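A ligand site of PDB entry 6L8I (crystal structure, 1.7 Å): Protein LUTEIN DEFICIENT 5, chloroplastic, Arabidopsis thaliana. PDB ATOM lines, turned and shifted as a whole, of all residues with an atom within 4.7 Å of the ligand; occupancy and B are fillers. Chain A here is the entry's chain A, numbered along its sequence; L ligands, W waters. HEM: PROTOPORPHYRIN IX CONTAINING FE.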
ATOM      1  N   LYS A  98      18.444   4.296 -14.589  1.00  0.00           N
ATOM      2  CA  LYS A  98      17.009   4.210 -14.819  1.00  0.00           C
ATOM      3  C   LYS A  98      16.206   5.179 -13.948  1.00  0.00           C
ATOM      4  O   LYS A  98      14.982   5.278 -14.098  1.00  0.00           O
ATOM      5  CB  LYS A  98      16.517   2.765 -14.609  1.00  0.00           C
ATOM      6  CG  LYS A  98      17.052   1.781 -15.644  1.00  0.00           C
ATOM      7  CD  LYS A  98      16.733   2.245 -17.073  1.00  0.00           C
ATOM      8  CE  LYS A  98      16.825   1.079 -18.084  1.00  0.00           C
ATOM      9  NZ  LYS A  98      15.650   0.154 -17.970  1.00  0.00           N
ATOM     10  N   LEU A 101      12.391   5.203 -12.580  1.00  0.00           N
ATOM     11  CA  LEU A 101      11.793   3.940 -13.006  1.00  0.00           C
ATOM     12  C   LEU A 101      11.920   2.906 -11.897  1.00  0.00           C
ATOM     13  O   LEU A 101      11.018   2.086 -11.689  1.00  0.00           O
ATOM     14  CB  LEU A 101      12.479   3.404 -14.287  1.00  0.00           C
ATOM     15  CG  LEU A 101      11.849   2.190 -14.962  1.00  0.00           C
ATOM     16  CD1 LEU A 101      10.435   2.533 -15.410  1.00  0.00           C
ATOM     17  CD2 LEU A 101      12.685   1.708 -16.150  1.00  0.00           C
ATOM     18  N   LEU A 113      15.847  -7.023 -14.142  1.00  0.00           N
ATOM     19  CA  LEU A 113      16.642  -6.334 -15.146  1.00  0.00           C
ATOM     20  C   LEU A 113      16.198  -4.902 -15.446  1.00  0.00           C
ATOM     21  O   LEU A 113      17.035  -4.007 -15.606  1.00  0.00           O
ATOM     22  CB  LEU A 113      16.702  -7.140 -16.448  1.00  0.00           C
ATOM     23  CG  LEU A 113      17.729  -8.263 -16.499  1.00  0.00           C
ATOM     24  CD1 LEU A 113      17.668  -8.971 -17.825  1.00  0.00           C
ATOM     25  CD2 LEU A 113      19.122  -7.700 -16.244  1.00  0.00           C
ATOM     26  N   ILE A 114      14.893  -4.692 -15.531  1.00  0.00           N
ATOM     27  CA  ILE A 114      14.363  -3.400 -15.965  1.00  0.00           C
ATOM     28  C   ILE A 114      14.775  -2.210 -15.071  1.00  0.00           C
ATOM     29  O   ILE A 114      15.337  -1.241 -15.586  1.00  0.00           O
ATOM     30  CB  ILE A 114      12.829  -3.461 -16.211  1.00  0.00           C
ATOM     31  CG1 ILE A 114      12.535  -4.230 -17.504  1.00  0.00           C
ATOM     32  CG2 ILE A 114      12.253  -2.062 -16.307  1.00  0.00           C
ATOM     33  CD1 ILE A 114      11.065  -4.655 -17.675  1.00  0.00           C
ATOM     34  N   TRP A 121      22.876  -5.271 -12.612  1.00  0.00           N
ATOM     35  CA  TRP A 121      22.363  -5.316 -13.982  1.00  0.00           C
ATOM     36  C   TRP A 121      23.260  -6.136 -14.918  1.00  0.00           C
ATOM     37  O   TRP A 121      22.800  -7.061 -15.569  1.00  0.00           O
ATOM     38  CB  TRP A 121      22.153  -3.896 -14.559  1.00  0.00           C
ATOM     39  CG  TRP A 121      21.850  -4.002 -16.023  1.00  0.00           C
ATOM     40  CD1 TRP A 121      20.662  -4.364 -16.589  1.00  0.00           C
ATOM     41  CD2 TRP A 121      22.773  -3.798 -17.108  1.00  0.00           C
ATOM     42  NE1 TRP A 121      20.775  -4.393 -17.953  1.00  0.00           N
ATOM     43  CE2 TRP A 121      22.057  -4.062 -18.299  1.00  0.00           C
ATOM     44  CE3 TRP A 121      24.113  -3.423 -17.194  1.00  0.00           C
ATOM     45  CZ2 TRP A 121      22.644  -3.950 -19.554  1.00  0.00           C
ATOM     46  CZ3 TRP A 121      24.698  -3.314 -18.439  1.00  0.00           C
ATOM     47  CH2 TRP A 121      23.967  -3.574 -19.612  1.00  0.00           C
ATOM     48  N   ARG A 125      22.032  -9.574 -16.729  1.00  0.00           N
ATOM     49  CA  ARG A 125      21.888  -9.543 -18.182  1.00  0.00           C
ATOM     50  C   ARG A 125      22.733 -10.646 -18.834  1.00  0.00           C
ATOM     51  O   ARG A 125      22.260 -11.373 -19.700  1.00  0.00           O
ATOM     52  CB  ARG A 125      22.300  -8.166 -18.727  1.00  0.00           C
ATOM     53  CG  ARG A 125      22.302  -8.086 -20.237  1.00  0.00           C
ATOM     54  CD  ARG A 125      21.196  -7.201 -20.750  1.00  0.00           C
ATOM     55  NE  ARG A 125      21.173  -7.118 -22.201  1.00  0.00           N
ATOM     56  CZ  ARG A 125      20.234  -6.471 -22.899  1.00  0.00           C
ATOM     57  NH1 ARG A 125      19.244  -5.841 -22.272  1.00  0.00           N
ATOM     58  NH2 ARG A 125      20.297  -6.451 -24.230  1.00  0.00           N
ATOM     59  N   LEU A 132      17.681 -17.096 -24.167  1.00  0.00           N
ATOM     60  CA  LEU A 132      16.846 -16.811 -25.322  1.00  0.00           C
ATOM     61  C   LEU A 132      17.571 -17.088 -26.628  1.00  0.00           C
ATOM     62  O   LEU A 132      17.624 -16.247 -27.524  1.00  0.00           O
ATOM     63  CB  LEU A 132      16.340 -15.365 -25.250  1.00  0.00           C
ATOM     64  CG  LEU A 132      15.348 -15.198 -24.101  1.00  0.00           C
ATOM     65  CD1 LEU A 132      15.967 -14.457 -22.908  1.00  0.00           C
ATOM     66  CD2 LEU A 132      14.092 -14.473 -24.609  1.00  0.00           C
ATOM     67  N   ILE A 179       3.346 -15.838 -21.774  1.00  0.00           N
ATOM     68  CA  ILE A 179       4.560 -15.469 -21.062  1.00  0.00           C
ATOM     69  C   ILE A 179       4.797 -16.356 -19.833  1.00  0.00           C
ATOM     70  O   ILE A 179       5.932 -16.642 -19.511  1.00  0.00           O
ATOM     71  CB  ILE A 179       4.598 -13.941 -20.698  1.00  0.00           C
ATOM     72  CG1 ILE A 179       6.041 -13.525 -20.376  1.00  0.00           C
ATOM     73  CG2 ILE A 179       3.646 -13.600 -19.567  1.00  0.00           C
ATOM     74  CD1 ILE A 179       6.976 -13.553 -21.564  1.00  0.00           C
ATOM     75  N   ILE A 275      12.675 -20.457 -19.703  1.00  0.00           N
ATOM     76  CA  ILE A 275      13.857 -19.696 -19.327  1.00  0.00           C
ATOM     77  C   ILE A 275      14.322 -20.080 -17.916  1.00  0.00           C
ATOM     78  O   ILE A 275      15.524 -20.215 -17.675  1.00  0.00           O
ATOM     79  CB  ILE A 275      13.565 -18.188 -19.420  1.00  0.00           C
ATOM     80  CG1 ILE A 275      13.383 -17.804 -20.891  1.00  0.00           C
ATOM     81  CG2 ILE A 275      14.697 -17.377 -18.767  1.00  0.00           C
ATOM     82  CD1 ILE A 275      12.844 -16.374 -21.097  1.00  0.00           C
ATOM     83  N   THR A 297      10.035  -9.943 -13.294  1.00  0.00           N
ATOM     84  CA  THR A 297      10.369  -8.869 -14.229  1.00  0.00           C
ATOM     85  C   THR A 297      10.036  -9.286 -15.658  1.00  0.00           C
ATOM     86  O   THR A 297       9.402  -8.539 -16.393  1.00  0.00           O
ATOM     87  CB  THR A 297      11.837  -8.499 -14.126  1.00  0.00           C
ATOM     88  OG1 THR A 297      12.074  -7.934 -12.829  1.00  0.00           O
ATOM     89  CG2 THR A 297      12.204  -7.472 -15.193  1.00  0.00           C
ATOM     90  N   MET A 298      10.437 -10.498 -16.043  1.00  0.00           N
ATOM     91  CA  MET A 298      10.150 -10.948 -17.406  1.00  0.00           C
ATOM     92  C   MET A 298       8.655 -11.178 -17.625  1.00  0.00           C
ATOM     93  O   MET A 298       8.136 -10.941 -18.718  1.00  0.00           O
ATOM     94  CB  MET A 298      10.965 -12.205 -17.746  1.00  0.00           C
ATOM     95  CG  MET A 298      12.432 -11.878 -18.006  1.00  0.00           C
ATOM     96  SD  MET A 298      13.419 -13.345 -18.352  1.00  0.00           S
ATOM     97  CE  MET A 298      13.691 -13.937 -16.682  1.00  0.00           C
ATOM     98  N   ALA A 301       7.376  -7.658 -18.139  1.00  0.00           N
ATOM     99  CA  ALA A 301       7.936  -7.149 -19.377  1.00  0.00           C
ATOM    100  C   ALA A 301       7.290  -7.697 -20.650  1.00  0.00           C
ATOM    101  O   ALA A 301       7.153  -6.985 -21.638  1.00  0.00           O
ATOM    102  CB  ALA A 301       9.437  -7.393 -19.413  1.00  0.00           C
ATOM    103  N   GLY A 302       6.926  -8.985 -20.644  1.00  0.00           N
ATOM    104  CA  GLY A 302       6.441  -9.618 -21.849  1.00  0.00           C
ATOM    105  C   GLY A 302       4.938  -9.846 -21.911  1.00  0.00           C
ATOM    106  O   GLY A 302       4.449 -10.452 -22.854  1.00  0.00           O
ATOM    107  N   THR A 305       2.792  -5.523 -22.732  1.00  0.00           N
ATOM    108  CA  THR A 305       3.424  -4.976 -23.931  1.00  0.00           C
ATOM    109  C   THR A 305       2.810  -5.605 -25.198  1.00  0.00           C
ATOM    110  O   THR A 305       2.243  -4.889 -26.032  1.00  0.00           O
ATOM    111  CB  THR A 305       4.946  -5.239 -23.924  1.00  0.00           C
ATOM    112  OG1 THR A 305       5.171  -6.620 -23.578  1.00  0.00           O
ATOM    113  CG2 THR A 305       5.653  -4.333 -22.900  1.00  0.00           C
ATOM    114  N   SER A 306       2.898  -6.926 -25.347  1.00  0.00           N
ATOM    115  CA  SER A 306       2.322  -7.576 -26.515  1.00  0.00           C
ATOM    116  C   SER A 306       0.799  -7.485 -26.537  1.00  0.00           C
ATOM    117  O   SER A 306       0.194  -7.399 -27.595  1.00  0.00           O
ATOM    118  CB  SER A 306       2.778  -9.035 -26.635  1.00  0.00           C
ATOM    119  OG  SER A 306       4.131  -9.095 -27.050  1.00  0.00           O
ATOM    120  N   VAL A 309       0.297  -4.268 -28.149  1.00  0.00           N
ATOM    121  CA  VAL A 309       0.670  -4.335 -29.557  1.00  0.00           C
ATOM    122  C   VAL A 309      -0.446  -4.967 -30.382  1.00  0.00           C
ATOM    123  O   VAL A 309      -0.841  -4.440 -31.429  1.00  0.00           O
ATOM    124  CB  VAL A 309       2.002  -5.091 -29.764  1.00  0.00           C
ATOM    125  CG1 VAL A 309       2.266  -5.291 -31.256  1.00  0.00           C
ATOM    126  CG2 VAL A 309       3.144  -4.311 -29.148  1.00  0.00           C
ATOM    127  N   LEU A 359       3.734  -0.813 -33.859  1.00  0.00           N
ATOM    128  CA  LEU A 359       4.643  -0.384 -32.800  1.00  0.00           C
ATOM    129  C   LEU A 359       5.129   1.044 -33.026  1.00  0.00           C
ATOM    130  O   LEU A 359       5.417   1.774 -32.076  1.00  0.00           O
ATOM    131  CB  LEU A 359       5.820  -1.359 -32.645  1.00  0.00           C
ATOM    132  CG  LEU A 359       5.577  -2.469 -31.614  1.00  0.00           C
ATOM    133  CD1 LEU A 359       6.573  -3.627 -31.787  1.00  0.00           C
ATOM    134  CD2 LEU A 359       5.682  -1.926 -30.195  1.00  0.00           C
ATOM    135  N   GLN A 364       5.327   0.840 -26.914  1.00  0.00           N
ATOM    136  CA  GLN A 364       5.131   0.262 -25.598  1.00  0.00           C
ATOM    137  C   GLN A 364       6.487   0.120 -24.939  1.00  0.00           C
ATOM    138  O   GLN A 364       7.235  -0.795 -25.265  1.00  0.00           O
ATOM    139  CB  GLN A 364       4.462  -1.125 -25.723  1.00  0.00           C
ATOM    140  CG  GLN A 364       3.252  -1.169 -26.654  1.00  0.00           C
ATOM    141  CD  GLN A 364       2.104  -0.259 -26.170  1.00  0.00           C
ATOM    142  OE1 GLN A 364       1.913  -0.071 -24.972  1.00  0.00           O
ATOM    143  NE2 GLN A 364       1.342   0.301 -27.115  1.00  0.00           N
ATOM    144  N   PRO A 365       6.838   1.007 -24.015  1.00  0.00           N
ATOM    145  CA  PRO A 365       6.081   2.158 -23.520  1.00  0.00           C
ATOM    146  C   PRO A 365       6.252   3.357 -24.438  1.00  0.00           C
ATOM    147  O   PRO A 365       7.127   3.388 -25.305  1.00  0.00           O
ATOM    148  CB  PRO A 365       6.750   2.453 -22.182  1.00  0.00           C
ATOM    149  CG  PRO A 365       8.177   2.072 -22.401  1.00  0.00           C
ATOM    150  CD  PRO A 365       8.161   0.902 -23.353  1.00  0.00           C
ATOM    151  N   LEU A 368      10.532   6.471 -22.386  1.00  0.00           N
ATOM    152  CA  LEU A 368      11.626   5.764 -21.721  1.00  0.00           C
ATOM    153  C   LEU A 368      12.179   6.699 -20.662  1.00  0.00           C
ATOM    154  O   LEU A 368      12.256   7.919 -20.873  1.00  0.00           O
ATOM    155  CB  LEU A 368      12.738   5.413 -22.710  1.00  0.00           C
ATOM    156  CG  LEU A 368      12.305   4.422 -23.788  1.00  0.00           C
ATOM    157  CD1 LEU A 368      13.417   4.187 -24.788  1.00  0.00           C
ATOM    158  CD2 LEU A 368      11.883   3.110 -23.132  1.00  0.00           C
ATOM    159  N   ARG A 370      15.134   7.904 -17.855  1.00  0.00           N
ATOM    160  CA  ARG A 370      16.531   7.862 -17.414  1.00  0.00           C
ATOM    161  C   ARG A 370      16.773   8.978 -16.411  1.00  0.00           C
ATOM    162  O   ARG A 370      15.926   9.835 -16.220  1.00  0.00           O
ATOM    163  CB  ARG A 370      17.487   8.060 -18.588  1.00  0.00           C
ATOM    164  CG  ARG A 370      17.458   6.961 -19.662  1.00  0.00           C
ATOM    165  CD  ARG A 370      17.959   5.636 -19.107  1.00  0.00           C
ATOM    166  NE  ARG A 370      18.134   4.597 -20.137  1.00  0.00           N
ATOM    167  CZ  ARG A 370      17.182   3.743 -20.514  1.00  0.00           C
ATOM    168  NH1 ARG A 370      15.965   3.806 -19.981  1.00  0.00           N
ATOM    169  NH2 ARG A 370      17.450   2.820 -21.437  1.00  0.00           N
ATOM    170  N   LEU A 431      12.186   3.074 -32.179  1.00  0.00           N
ATOM    171  CA  LEU A 431      12.740   2.343 -31.044  1.00  0.00           C
ATOM    172  C   LEU A 431      11.724   1.404 -30.406  1.00  0.00           C
ATOM    173  O   LEU A 431      11.492   1.492 -29.193  1.00  0.00           O
ATOM    174  CB  LEU A 431      13.166   3.314 -29.930  1.00  0.00           C
ATOM    175  CG  LEU A 431      14.002   4.540 -30.213  1.00  0.00           C
ATOM    176  CD1 LEU A 431      14.208   5.284 -28.895  1.00  0.00           C
ATOM    177  CD2 LEU A 431      15.317   4.107 -30.803  1.00  0.00           C
ATOM    178  N   PRO A 432      11.123   0.522 -31.197  1.00  0.00           N
ATOM    179  CA  PRO A 432      10.090  -0.404 -30.698  1.00  0.00           C
ATOM    180  C   PRO A 432      10.542  -1.197 -29.476  1.00  0.00           C
ATOM    181  O   PRO A 432       9.750  -1.465 -28.580  1.00  0.00           O
ATOM    182  CB  PRO A 432       9.856  -1.329 -31.881  1.00  0.00           C
ATOM    183  CG  PRO A 432      11.134  -1.269 -32.675  1.00  0.00           C
ATOM    184  CD  PRO A 432      11.515   0.189 -32.567  1.00  0.00           C
ATOM    185  N   PHE A 433      11.830  -1.534 -29.430  1.00  0.00           N
ATOM    186  CA  PHE A 433      12.373  -2.330 -28.325  1.00  0.00           C
ATOM    187  C   PHE A 433      13.498  -1.625 -27.585  1.00  0.00           C
ATOM    188  O   PHE A 433      14.319  -2.265 -26.914  1.00  0.00           O
ATOM    189  CB  PHE A 433      12.801  -3.715 -28.836  1.00  0.00           C
ATOM    190  CG  PHE A 433      11.655  -4.520 -29.353  1.00  0.00           C
ATOM    191  CD1 PHE A 433      10.818  -5.193 -28.472  1.00  0.00           C
ATOM    192  CD2 PHE A 433      11.397  -4.586 -30.710  1.00  0.00           C
ATOM    193  CE1 PHE A 433       9.732  -5.931 -28.946  1.00  0.00           C
ATOM    194  CE2 PHE A 433      10.324  -5.331 -31.194  1.00  0.00           C
ATOM    195  CZ  PHE A 433       9.497  -5.991 -30.317  1.00  0.00           C
ATOM    196  N   GLY A 434      13.525  -0.300 -27.695  1.00  0.00           N
ATOM    197  CA  GLY A 434      14.585   0.472 -27.079  1.00  0.00           C
ATOM    198  C   GLY A 434      15.870   0.433 -27.888  1.00  0.00           C
ATOM    199  O   GLY A 434      15.859   0.209 -29.102  1.00  0.00           O
ATOM    200  N   PRO A 437      22.612  -0.558 -24.656  1.00  0.00           N
ATOM    201  CA  PRO A 437      22.820  -1.713 -23.773  1.00  0.00           C
ATOM    202  C   PRO A 437      21.578  -2.191 -23.032  1.00  0.00           C
ATOM    203  O   PRO A 437      21.552  -3.365 -22.657  1.00  0.00           O
ATOM    204  CB  PRO A 437      23.864  -1.206 -22.766  1.00  0.00           C
ATOM    205  CG  PRO A 437      24.494  -0.020 -23.418  1.00  0.00           C
ATOM    206  CD  PRO A 437      23.455   0.588 -24.289  1.00  0.00           C
ATOM    207  N   ARG A 438      20.577  -1.328 -22.844  1.00  0.00           N
ATOM    208  CA  ARG A 438      19.379  -1.693 -22.083  1.00  0.00           C
ATOM    209  C   ARG A 438      18.226  -2.132 -22.991  1.00  0.00           C
ATOM    210  O   ARG A 438      17.102  -2.252 -22.517  1.00  0.00           O
ATOM    211  CB  ARG A 438      18.907  -0.519 -21.204  1.00  0.00           C
ATOM    212  CG  ARG A 438      19.985   0.016 -20.256  1.00  0.00           C
ATOM    213  CD  ARG A 438      20.548  -1.111 -19.396  1.00  0.00           C
ATOM    214  NE  ARG A 438      19.533  -1.675 -18.518  1.00  0.00           N
ATOM    215  CZ  ARG A 438      19.370  -1.338 -17.241  1.00  0.00           C
ATOM    216  NH1 ARG A 438      20.169  -0.424 -16.671  1.00  0.00           N
ATOM    217  NH2 ARG A 438      18.407  -1.907 -16.532  1.00  0.00           N
ATOM    218  N   LYS A 439      18.520  -2.352 -24.268  1.00  0.00           N
ATOM    219  CA  LYS A 439      17.516  -2.783 -25.234  1.00  0.00           C
ATOM    220  C   LYS A 439      16.813  -4.071 -24.777  1.00  0.00           C
ATOM    221  O   LYS A 439      17.432  -4.942 -24.175  1.00  0.00           O
ATOM    222  CB  LYS A 439      18.173  -3.008 -26.607  1.00  0.00           C
ATOM    223  CG  LYS A 439      17.231  -3.443 -27.697  1.00  0.00           C
ATOM    224  CD  LYS A 439      17.945  -3.647 -29.008  1.00  0.00           C
ATOM    225  CE  LYS A 439      16.959  -4.035 -30.096  1.00  0.00           C
ATOM    226  NZ  LYS A 439      17.640  -4.148 -31.411  1.00  0.00           N
ATOM    227  N   CYS A 440      15.529  -4.179 -25.072  1.00  0.00           N
ATOM    228  CA  CYS A 440      14.750  -5.372 -24.777  1.00  0.00           C
ATOM    229  C   CYS A 440      15.452  -6.681 -25.159  1.00  0.00           C
ATOM    230  O   CYS A 440      15.922  -6.841 -26.282  1.00  0.00           O
ATOM    231  CB  CYS A 440      13.437  -5.287 -25.559  1.00  0.00           C
ATOM    232  SG  CYS A 440      12.293  -6.594 -25.234  1.00  0.00           S
ATOM    233  N   ILE A 441      15.503  -7.618 -24.211  1.00  0.00           N
ATOM    234  CA  ILE A 441      16.028  -8.967 -24.498  1.00  0.00           C
ATOM    235  C   ILE A 441      15.002  -9.862 -25.191  1.00  0.00           C
ATOM    236  O   ILE A 441      15.363 -10.926 -25.726  1.00  0.00           O
ATOM    237  CB  ILE A 441      16.535  -9.667 -23.216  1.00  0.00           C
ATOM    238  CG1 ILE A 441      15.383  -9.916 -22.241  1.00  0.00           C
ATOM    239  CG2 ILE A 441      17.650  -8.876 -22.572  1.00  0.00           C
ATOM    240  CD1 ILE A 441      15.733 -10.889 -21.125  1.00  0.00           C
ATOM    241  N   GLY A 442      13.743  -9.449 -25.200  1.00  0.00           N
ATOM    242  CA  GLY A 442      12.690 -10.246 -25.799  1.00  0.00           C
ATOM    243  C   GLY A 442      12.236  -9.721 -27.148  1.00  0.00           C
ATOM    244  O   GLY A 442      11.112 -10.000 -27.568  1.00  0.00           O
ATOM    245  N   PHE A 445      11.689 -12.720 -29.591  1.00  0.00           N
ATOM    246  CA  PHE A 445      10.575 -13.448 -28.961  1.00  0.00           C
ATOM    247  C   PHE A 445       9.247 -12.751 -29.260  1.00  0.00           C
ATOM    248  O   PHE A 445       8.332 -13.359 -29.817  1.00  0.00           O
ATOM    249  CB  PHE A 445      10.830 -13.514 -27.450  1.00  0.00           C
ATOM    250  CG  PHE A 445       9.799 -14.268 -26.648  1.00  0.00           C
ATOM    251  CD1 PHE A 445       8.529 -13.741 -26.415  1.00  0.00           C
ATOM    252  CD2 PHE A 445      10.109 -15.509 -26.084  1.00  0.00           C
ATOM    253  CE1 PHE A 445       7.606 -14.413 -25.650  1.00  0.00           C
ATOM    254  CE2 PHE A 445       9.179 -16.201 -25.326  1.00  0.00           C
ATOM    255  CZ  PHE A 445       7.924 -15.647 -25.114  1.00  0.00           C
ATOM    256  N   ALA A 446       9.159 -11.473 -28.899  1.00  0.00           N
ATOM    257  CA  ALA A 446       7.901 -10.739 -29.032  1.00  0.00           C
ATOM    258  C   ALA A 446       7.521 -10.452 -30.481  1.00  0.00           C
ATOM    259  O   ALA A 446       6.342 -10.483 -30.837  1.00  0.00           O
ATOM    260  CB  ALA A 446       7.966  -9.428 -28.210  1.00  0.00           C
ATOM    261  N   ASN A 450       3.913 -11.833 -31.844  1.00  0.00           N
ATOM    262  CA  ASN A 450       2.862 -10.992 -32.409  1.00  0.00           C
ATOM    263  C   ASN A 450       2.566 -11.303 -33.874  1.00  0.00           C
ATOM    264  O   ASN A 450       1.411 -11.319 -34.284  1.00  0.00           O
ATOM    265  CB  ASN A 450       3.149  -9.514 -32.126  1.00  0.00           C
ATOM    266  CG  ASN A 450       3.068  -9.213 -30.637  1.00  0.00           C
ATOM    267  OD1 ASN A 450       2.043  -9.499 -30.004  1.00  0.00           O
ATOM    268  ND2 ASN A 450       4.145  -8.699 -30.057  1.00  0.00           N
HETATM  269  CHA HEM L   1      13.346  -3.890 -21.888  1.00  0.00           C
HETATM  270  CHB HEM L   1       9.783  -3.251 -25.091  1.00  0.00           C
HETATM  271  CHC HEM L   1       8.494  -7.907 -24.719  1.00  0.00           C
HETATM  272  CHD HEM L   1      11.964  -8.577 -21.386  1.00  0.00           C
HETATM  273  C1A HEM L   1      12.533  -3.324 -22.833  1.00  0.00           C
HETATM  274  C2A HEM L   1      12.639  -1.975 -23.343  1.00  0.00           C
HETATM  275  C3A HEM L   1      11.647  -1.804 -24.226  1.00  0.00           C
HETATM  276  C4A HEM L   1      10.877  -3.018 -24.296  1.00  0.00           C
HETATM  277  CMA HEM L   1      11.358  -0.516 -25.049  1.00  0.00           C
HETATM  278  CAA HEM L   1      13.733  -0.950 -22.937  1.00  0.00           C
HETATM  279  CBA HEM L   1      13.274  -0.137 -21.729  1.00  0.00           C
HETATM  280  CGA HEM L   1      14.338   0.875 -21.324  1.00  0.00           C
HETATM  281  O1A HEM L   1      15.389   0.978 -22.001  1.00  0.00           O
HETATM  282  O2A HEM L   1      14.123   1.549 -20.296  1.00  0.00           O
HETATM  283  C1B HEM L   1       9.121  -4.439 -25.267  1.00  0.00           C
HETATM  284  C2B HEM L   1       8.007  -4.653 -26.147  1.00  0.00           C
HETATM  285  C3B HEM L   1       7.631  -5.954 -26.051  1.00  0.00           C
HETATM  286  C4B HEM L   1       8.519  -6.595 -25.109  1.00  0.00           C
HETATM  287  CMB HEM L   1       7.389  -3.545 -27.035  1.00  0.00           C
HETATM  288  CAB HEM L   1       6.497  -6.682 -26.789  1.00  0.00           C
HETATM  289  CBB HEM L   1       5.943  -6.250 -27.932  1.00  0.00           C
HETATM  290  C1C HEM L   1       9.398  -8.498 -23.844  1.00  0.00           C
HETATM  291  C2C HEM L   1       9.540  -9.908 -23.621  1.00  0.00           C
HETATM  292  C3C HEM L   1      10.491 -10.114 -22.694  1.00  0.00           C
HETATM  293  C4C HEM L   1      10.987  -8.805 -22.322  1.00  0.00           C
HETATM  294  CMC HEM L   1       8.675 -10.940 -24.367  1.00  0.00           C
HETATM  295  CAC HEM L   1      11.045 -11.433 -22.102  1.00  0.00           C
HETATM  296  CBC HEM L   1      10.873 -12.653 -22.627  1.00  0.00           C
HETATM  297  C1D HEM L   1      12.613  -7.382 -21.201  1.00  0.00           C
HETATM  298  C2D HEM L   1      13.666  -7.185 -20.234  1.00  0.00           C
HETATM  299  C3D HEM L   1      14.082  -5.741 -20.388  1.00  0.00           C
HETATM  300  C4D HEM L   1      13.256  -5.190 -21.446  1.00  0.00           C
HETATM  301  CMD HEM L   1      14.259  -8.171 -19.223  1.00  0.00           C
HETATM  302  CAD HEM L   1      15.204  -5.038 -19.596  1.00  0.00           C
HETATM  303  CBD HEM L   1      16.519  -5.256 -20.340  1.00  0.00           C
HETATM  304  CGD HEM L   1      17.650  -4.682 -19.528  1.00  0.00           C
HETATM  305  O1D HEM L   1      18.747  -5.309 -19.511  1.00  0.00           O
HETATM  306  O2D HEM L   1      17.460  -3.616 -18.898  1.00  0.00           O
HETATM  307  NA  HEM L   1      11.441  -3.940 -23.424  1.00  0.00           N
HETATM  308  NB  HEM L   1       9.403  -5.638 -24.634  1.00  0.00           N
HETATM  309  NC  HEM L   1      10.310  -7.851 -23.032  1.00  0.00           N
HETATM  310  ND  HEM L   1      12.386  -6.185 -21.886  1.00  0.00           N
HETATM  311 FE   HEM L   1      10.963  -5.925 -23.327  1.00  0.00          FE
HETATM  312  O   HOH W   1       5.533 -10.394 -25.398  1.00  0.00           O
HETATM  313  O   HOH W   2      11.695   2.284 -26.915  1.00  0.00           O
HETATM  314  O   HOH W   3      12.150   3.372 -19.302  1.00  0.00           O
HETATM  315  O   HOH W   4       9.267  -5.156 -21.703  1.00  0.00           O
HETATM  316  O   HOH W   5      15.774  -1.731 -19.979  1.00  0.00           O
HETATM  317  O   HOH W   6      16.648   0.710 -24.294  1.00  0.00           O
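O of Phe 433 sits at hydrogen-bond distance from N of Cys 440 (2.9 Å).
SG of Cys 440 sits close to N of Gly 442, at 3.2 Å.
The backbone carbonyl oxygen (O) of Lys 439 sits at hydrogen-bond distance from the guanidinium group (NH1) of Arg 125, 2.8 Å away.
O of Leu 113 sits at hydrogen-bond distance from NH2 of Arg 438 (2.7 Å).
O of Ile 114 sits at hydrogen-bond distance from NH2 of Arg 438, at 3.3 Å.
O of Ile 114 sits at hydrogen-bond distance from NZ of Lys 98, at 2.8 Å.
ND2 of Asn 450 sits at hydrogen-bond distance from OG of Ser 306 (3.0 Å).
The backbone carbonyl oxygen (O) of Ala 301 is in hydrogen-bond range of the side-chain hydroxyl (OG1) of Thr 305.
Water W6 bridges an oxygen (O1A) of the ligand (2.6 Å) and the backbone carbonyl oxygen of Arg 438 (3.5 Å).
Water W5 lies within hydrogen-bond range of O2D of the ligand (2.8 Å), NZ of Lys 98 (2.8 Å) and O of Arg 438 (2.9 Å).
Water W1 lies within hydrogen-bond range of OG of Ser 306 (2.5 Å) and O of Gly 302 (2.8 Å).
An iron atom (FE) of the ligand is bound by the side-chain sulfur (SG) of Cys 440, 2.4 Å away.
NE1 of Trp 121 lies within hydrogen-bond range of O1D of the ligand (2.7 Å).
NH2 of Arg 370 lies within salt-bridge range of O1A of the ligand, at 2.8 Å.
The guanidinium group of Arg 125 is in salt-bridge range of an oxygen (O1D) of the ligand, at 2.9 Å.
O2D of the ligand is in salt-bridge range of NE of Arg 438.
The side-chain amino group of Lys 98 lies within salt-bridge range of an oxygen (O2A) of the ligand (3.1 Å).
The backbone carbonyl oxygen (O) of Leu 113 lies close to an oxygen (O2D) of the ligand, 3.3 Å away.
CG1 of Ile 114 touches CAD of the ligand, 3.5 Å away.
Ala 301 touches the ligand.
Gly 302 touches the ligand.
OG1 of Thr 305 touches CAB of the ligand, 3.5 Å away.
Ser 306 touches the ligand.
CG2 of Val 309 touches CBB of the ligand, 3.6 Å away.
Leu 359 touches the ligand.
Gln 364 touches the ligand.
Pro 365 touches the ligand.
CD2 of Leu 368 touches CGA of the ligand, 3.8 Å away.
Pro 432 touches the ligand (O to CMB, 3.5 Å).
Phe 433 touches the ligand.
N of Gly 434 touches CMA of the ligand (3.4 Å).
O of Lys 439 touches CBD of the ligand, 3.95 Å away.
Ile 441 touches the ligand (CD1 to CMD, 3.6 Å).
Gly 442 touches the ligand (CA to C3C, 3.8 Å).
Phe 445 touches the ligand.
CB of Ala 446 touches CAB of the ligand, 3.4 Å away.
Asn 450 touches the ligand.
Hydrophobic or aromatic side chains within 4 Å of the ligand: Leu 113, Ile 114, Trp 121, Ala 301, Val 309, Leu 359, Pro 365, Leu 368, Phe 433, Ile 441, Phe 445 and Ala 446.
Within 4 Å of the ligand: Lys 98, Leu 113, Ile 114, Trp 121, Arg 125, Ala 301, Gly 302, Thr 305, Ser 306, Val 309, Leu 359, Gln 364, Pro 365, Leu 368, Arg 370, Pro 432, Phe 433, Gly 434, Arg 438, Lys 439, Cys 440, Ile 441, Gly 442, Phe 445, Ala 446 and Asn 450.
The nearest printed residue that does not touch the ligand is Ile 179 (4.1 Å).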
